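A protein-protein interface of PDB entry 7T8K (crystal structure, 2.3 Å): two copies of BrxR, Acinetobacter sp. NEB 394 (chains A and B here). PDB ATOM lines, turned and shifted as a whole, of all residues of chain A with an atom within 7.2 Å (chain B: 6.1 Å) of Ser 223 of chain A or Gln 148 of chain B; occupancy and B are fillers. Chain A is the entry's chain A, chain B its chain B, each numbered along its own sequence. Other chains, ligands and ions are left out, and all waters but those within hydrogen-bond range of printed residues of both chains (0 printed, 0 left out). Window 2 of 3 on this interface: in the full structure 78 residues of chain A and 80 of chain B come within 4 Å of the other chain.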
ATOM      1  N   LEU A 220     -19.716  -7.088  -5.572  1.00  0.00           N
ATOM      2  CA  LEU A 220     -18.526  -7.465  -6.326  1.00  0.00           C
ATOM      3  C   LEU A 220     -18.893  -7.872  -7.747  1.00  0.00           C
ATOM      4  O   LEU A 220     -19.989  -8.371  -8.008  1.00  0.00           O
ATOM      5  CB  LEU A 220     -17.782  -8.619  -5.650  1.00  0.00           C
ATOM      6  CG  LEU A 220     -17.423  -8.529  -4.170  1.00  0.00           C
ATOM      7  CD1 LEU A 220     -17.341  -9.926  -3.562  1.00  0.00           C
ATOM      8  CD2 LEU A 220     -16.111  -7.781  -3.997  1.00  0.00           C
ATOM      9  N   ASN A 221     -17.954  -7.666  -8.668  1.00  0.00           N
ATOM     10  CA  ASN A 221     -18.214  -8.066 -10.040  1.00  0.00           C
ATOM     11  C   ASN A 221     -18.162  -9.591 -10.166  1.00  0.00           C
ATOM     12  O   ASN A 221     -17.829 -10.314  -9.223  1.00  0.00           O
ATOM     13  CB  ASN A 221     -17.238  -7.376 -11.002  1.00  0.00           C
ATOM     14  CG  ASN A 221     -15.808  -7.894 -10.895  1.00  0.00           C
ATOM     15  OD1 ASN A 221     -15.566  -9.069 -10.616  1.00  0.00           O
ATOM     16  ND2 ASN A 221     -14.849  -7.012 -11.155  1.00  0.00           N
ATOM     17  N   SER A 222     -18.498 -10.075 -11.363  1.00  0.00           N
ATOM     18  CA  SER A 222     -18.695 -11.509 -11.563  1.00  0.00           C
ATOM     19  C   SER A 222     -17.411 -12.300 -11.330  1.00  0.00           C
ATOM     20  O   SER A 222     -17.445 -13.393 -10.752  1.00  0.00           O
ATOM     21  CB  SER A 222     -19.243 -11.763 -12.964  1.00  0.00           C
ATOM     22  OG  SER A 222     -20.647 -11.587 -12.979  1.00  0.00           O
ATOM     23  N   SER A 223     -16.269 -11.779 -11.778  1.00  0.00           N
ATOM     24  CA  SER A 223     -15.022 -12.507 -11.559  1.00  0.00           C
ATOM     25  C   SER A 223     -14.657 -12.531 -10.081  1.00  0.00           C
ATOM     26  O   SER A 223     -14.098 -13.520  -9.591  1.00  0.00           O
ATOM     27  CB  SER A 223     -13.893 -11.890 -12.382  1.00  0.00           C
ATOM     28  OG  SER A 223     -14.211 -11.908 -13.760  1.00  0.00           O
ATOM     29  N   GLN A 224     -14.963 -11.454  -9.356  1.00  0.00           N
ATOM     30  CA  GLN A 224     -14.689 -11.437  -7.922  1.00  0.00           C
ATOM     31  C   GLN A 224     -15.580 -12.423  -7.177  1.00  0.00           C
ATOM     32  O   GLN A 224     -15.128 -13.086  -6.236  1.00  0.00           O
ATOM     33  CB  GLN A 224     -14.872 -10.027  -7.368  1.00  0.00           C
ATOM     34  CG  GLN A 224     -13.803  -9.039  -7.812  1.00  0.00           C
ATOM     35  CD  GLN A 224     -14.188  -7.602  -7.517  1.00  0.00           C
ATOM     36  OE1 GLN A 224     -15.367  -7.245  -7.536  1.00  0.00           O
ATOM     37  NE2 GLN A 224     -13.193  -6.771  -7.236  1.00  0.00           N
ATOM     38  N   GLN A 225     -16.848 -12.538  -7.580  1.00  0.00           N
ATOM     39  CA  GLN A 225     -17.749 -13.460  -6.896  1.00  0.00           C
ATOM     40  C   GLN A 225     -17.333 -14.908  -7.105  1.00  0.00           C
ATOM     41  O   GLN A 225     -17.486 -15.735  -6.197  1.00  0.00           O
ATOM     42  CB  GLN A 225     -19.183 -13.256  -7.377  1.00  0.00           C
ATOM     43  CG  GLN A 225     -19.697 -11.848  -7.210  1.00  0.00           C
ATOM     44  CD  GLN A 225     -21.203 -11.780  -7.295  1.00  0.00           C
ATOM     45  OE1 GLN A 225     -21.894 -12.766  -7.033  1.00  0.00           O
ATOM     46  NE2 GLN A 225     -21.722 -10.616  -7.664  1.00  0.00           N
ATOM     47  N   ALA A 226     -16.804 -15.230  -8.287  1.00  0.00           N
ATOM     48  CA  ALA A 226     -16.315 -16.581  -8.530  1.00  0.00           C
ATOM     49  C   ALA A 226     -15.181 -16.918  -7.574  1.00  0.00           C
ATOM     50  O   ALA A 226     -15.059 -18.059  -7.112  1.00  0.00           O
ATOM     51  CB  ALA A 226     -15.858 -16.722  -9.982  1.00  0.00           C
ATOM     52  N   LEU A 227     -14.348 -15.926  -7.252  1.00  0.00           N
ATOM     53  CA  LEU A 227     -13.278 -16.147  -6.289  1.00  0.00           C
ATOM     54  C   LEU A 227     -13.839 -16.420  -4.898  1.00  0.00           C
ATOM     55  O   LEU A 227     -13.324 -17.280  -4.182  1.00  0.00           O
ATOM     56  CB  LEU A 227     -12.328 -14.949  -6.269  1.00  0.00           C
ATOM     57  CG  LEU A 227     -11.410 -14.768  -7.485  1.00  0.00           C
ATOM     58  CD1 LEU A 227     -10.272 -13.815  -7.157  1.00  0.00           C
ATOM     59  CD2 LEU A 227     -10.869 -16.104  -7.989  1.00  0.00           C
ATOM     60  N   VAL A 228     -14.886 -15.697  -4.490  1.00  0.00           N
ATOM     61  CA  VAL A 228     -15.531 -15.983  -3.207  1.00  0.00           C
ATOM     62  C   VAL A 228     -16.076 -17.407  -3.190  1.00  0.00           C
ATOM     63  O   VAL A 228     -15.918 -18.150  -2.208  1.00  0.00           O
ATOM     64  CB  VAL A 228     -16.642 -14.955  -2.931  1.00  0.00           C
ATOM     65  CG1 VAL A 228     -17.289 -15.208  -1.578  1.00  0.00           C
ATOM     66  CG2 VAL A 228     -16.080 -13.544  -3.006  1.00  0.00           C
ATOM     67  N   TYR B 141      -2.571 -17.895 -10.137  1.00  0.00           N
ATOM     68  CA  TYR B 141      -3.182 -17.213  -9.005  1.00  0.00           C
ATOM     69  C   TYR B 141      -4.217 -16.213  -9.498  1.00  0.00           C
ATOM     70  O   TYR B 141      -4.250 -15.847 -10.675  1.00  0.00           O
ATOM     71  CB  TYR B 141      -2.119 -16.504  -8.145  1.00  0.00           C
ATOM     72  CG  TYR B 141      -2.612 -15.988  -6.805  1.00  0.00           C
ATOM     73  CD1 TYR B 141      -2.870 -16.858  -5.756  1.00  0.00           C
ATOM     74  CD2 TYR B 141      -2.798 -14.627  -6.588  1.00  0.00           C
ATOM     75  CE1 TYR B 141      -3.310 -16.394  -4.530  1.00  0.00           C
ATOM     76  CE2 TYR B 141      -3.237 -14.150  -5.362  1.00  0.00           C
ATOM     77  CZ  TYR B 141      -3.492 -15.040  -4.338  1.00  0.00           C
ATOM     78  OH  TYR B 141      -3.930 -14.581  -3.117  1.00  0.00           O
ATOM     79  N   ALA B 142      -5.074 -15.780  -8.575  1.00  0.00           N
ATOM     80  CA  ALA B 142      -6.034 -14.715  -8.827  1.00  0.00           C
ATOM     81  C   ALA B 142      -6.354 -14.026  -7.508  1.00  0.00           C
ATOM     82  O   ALA B 142      -6.530 -14.691  -6.485  1.00  0.00           O
ATOM     83  CB  ALA B 142      -7.320 -15.245  -9.469  1.00  0.00           C
ATOM     84  N   SER B 143      -6.418 -12.697  -7.538  1.00  0.00           N
ATOM     85  CA  SER B 143      -6.715 -11.896  -6.358  1.00  0.00           C
ATOM     86  C   SER B 143      -7.979 -11.074  -6.587  1.00  0.00           C
ATOM     87  O   SER B 143      -8.507 -10.994  -7.699  1.00  0.00           O
ATOM     88  CB  SER B 143      -5.539 -10.977  -6.008  1.00  0.00           C
ATOM     89  OG  SER B 143      -5.473  -9.874  -6.897  1.00  0.00           O
ATOM     90  N   ASN B 146      -6.975  -8.312  -8.911  1.00  0.00           N
ATOM     91  CA  ASN B 146      -6.807  -8.831 -10.268  1.00  0.00           C
ATOM     92  C   ASN B 146      -7.425 -10.222 -10.290  1.00  0.00           C
ATOM     93  O   ASN B 146      -6.732 -11.236 -10.100  1.00  0.00           O
ATOM     94  CB  ASN B 146      -5.338  -8.852 -10.693  1.00  0.00           C
ATOM     95  CG  ASN B 146      -5.132  -9.531 -12.042  1.00  0.00           C
ATOM     96  OD1 ASN B 146      -6.085  -9.745 -12.791  1.00  0.00           O
ATOM     97  ND2 ASN B 146      -3.884  -9.870 -12.357  1.00  0.00           N
ATOM     98  N   PRO B 147      -8.731 -10.312 -10.532  1.00  0.00           N
ATOM     99  CA  PRO B 147      -9.438 -11.595 -10.429  1.00  0.00           C
ATOM    100  C   PRO B 147      -9.412 -12.420 -11.704  1.00  0.00           C
ATOM    101  O   PRO B 147     -10.170 -13.389 -11.803  1.00  0.00           O
ATOM    102  CB  PRO B 147     -10.874 -11.161 -10.098  1.00  0.00           C
ATOM    103  CG  PRO B 147     -11.011  -9.803 -10.699  1.00  0.00           C
ATOM    104  CD  PRO B 147      -9.641  -9.186 -10.792  1.00  0.00           C
ATOM    105  N   GLN B 148      -8.568 -12.064 -12.668  1.00  0.00           N
ATOM    106  CA  GLN B 148      -8.339 -12.919 -13.816  1.00  0.00           C
ATOM    107  C   GLN B 148      -7.122 -13.786 -13.532  1.00  0.00           C
ATOM    108  O   GLN B 148      -6.133 -13.324 -12.955  1.00  0.00           O
ATOM    109  CB  GLN B 148      -8.115 -12.080 -15.076  1.00  0.00           C
ATOM    110  CG  GLN B 148      -9.390 -11.682 -15.797  1.00  0.00           C
ATOM    111  CD  GLN B 148     -10.234 -10.704 -15.005  1.00  0.00           C
ATOM    112  OE1 GLN B 148     -11.450 -10.860 -14.908  1.00  0.00           O
ATOM    113  NE2 GLN B 148      -9.595  -9.685 -14.438  1.00  0.00           N
ATOM    114  N   TRP B 149      -7.196 -15.042 -13.949  1.00  0.00           N
ATOM    115  CA  TRP B 149      -6.153 -15.995 -13.604  1.00  0.00           C
ATOM    116  C   TRP B 149      -4.852 -15.619 -14.300  1.00  0.00           C
ATOM    117  O   TRP B 149      -4.834 -15.329 -15.501  1.00  0.00           O
ATOM    118  CB  TRP B 149      -6.612 -17.405 -13.949  1.00  0.00           C
ATOM    119  CG  TRP B 149      -7.788 -17.773 -13.094  1.00  0.00           C
ATOM    120  CD1 TRP B 149      -9.104 -17.759 -13.455  1.00  0.00           C
ATOM    121  CD2 TRP B 149      -7.755 -18.153 -11.712  1.00  0.00           C
ATOM    122  NE1 TRP B 149      -9.890 -18.128 -12.392  1.00  0.00           N
ATOM    123  CE2 TRP B 149      -9.087 -18.377 -11.310  1.00  0.00           C
ATOM    124  CE3 TRP B 149      -6.729 -18.339 -10.781  1.00  0.00           C
ATOM    125  CZ2 TRP B 149      -9.418 -18.775 -10.017  1.00  0.00           C
ATOM    126  CZ3 TRP B 149      -7.059 -18.735  -9.500  1.00  0.00           C
ATOM    127  CH2 TRP B 149      -8.392 -18.949  -9.129  1.00  0.00           C
ATOM    128  N   HIS B 150      -3.766 -15.596 -13.533  1.00  0.00           N
ATOM    129  CA  HIS B 150      -2.474 -15.183 -14.057  1.00  0.00           C
ATOM    130  C   HIS B 150      -1.367 -15.917 -13.320  1.00  0.00           C
ATOM    131  O   HIS B 150      -1.581 -16.501 -12.254  1.00  0.00           O
ATOM    132  CB  HIS B 150      -2.288 -13.668 -13.919  1.00  0.00           C
ATOM    133  CG  HIS B 150      -2.343 -13.188 -12.501  1.00  0.00           C
ATOM    134  ND1 HIS B 150      -3.531 -12.908 -11.858  1.00  0.00           N
ATOM    135  CD2 HIS B 150      -1.363 -12.951 -11.598  1.00  0.00           C
ATOM    136  CE1 HIS B 150      -3.277 -12.512 -10.623  1.00  0.00           C
ATOM    137  NE2 HIS B 150      -1.969 -12.529 -10.440  1.00  0.00           N
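Of chain B, only Pro 147 (3.9 Å) and Gln 148 (3.2 Å) come within 4 Å of Ser 223 of chain A. Printed residues of chain B within 4 Å of Leu 227 of chain A: Ala 142 (3.9 Å), Ser 143 (3.4 Å) and Trp 149 (3.7 Å). Of the printed residues of chain A, Ala 142 of chain B touches Leu 227. Of the printed residues of chain A, Ser 143 of chain B touches Leu 227 (3.4 Å). Gln 148 of chain B touches just one residue of chain A: Ser 223 (3.2 Å). Printed residues of chain A within 4 Å of Trp 149 of chain B: Leu 227 (3.7 Å). The nearest printed residue of chain B that does not touch Ser 223 of chain A is Ser 143 of chain B (6.4 Å). The nearest residue of chain A that does not touch Gln 148 of chain B is Leu 227 of chain A (6.0 Å).
No position is printed for both chains.
Of the 9 printed residues of chain A, 2 touch a printed residue of chain B. Among the printed residues, 5 pairs touch across the chains.
Among the printed residues, merely in contact across the chains: Ser 223 of chain A with Pro 147 of chain B (3.9 Å), Leu 227 of chain A with Ala 142 of chain B (3.9 Å), Leu 227 of chain A with Ser 143 of chain B (3.4 Å) and Leu 227 of chain A with Trp 149 of chain B (3.7 Å).
The side-chain amide oxygen (OD1) of Asn 221 of chain A sits at hydrogen-bond distance from the backbone NH (N) of Ser 223 of chain A, at 3.0 Å. N of Asn 146 of chain B lies within hydrogen-bond range of OG of Ser 143 of chain B (3.0 Å). OD1 of Asn 146 of chain B sits close to N of Gln 148 of chain B. The backbone carbonyl oxygen (O) of Gln 148 of chain B sits at hydrogen-bond distance from a ring nitrogen (ND1) of His 150 of chain B, 2.9 Å away.
The side-chain hydroxyl (OG) of Ser 223 of chain A sits at hydrogen-bond distance from the side-chain amide oxygen (OE1) of Gln 148 of chain B (3.2 Å).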
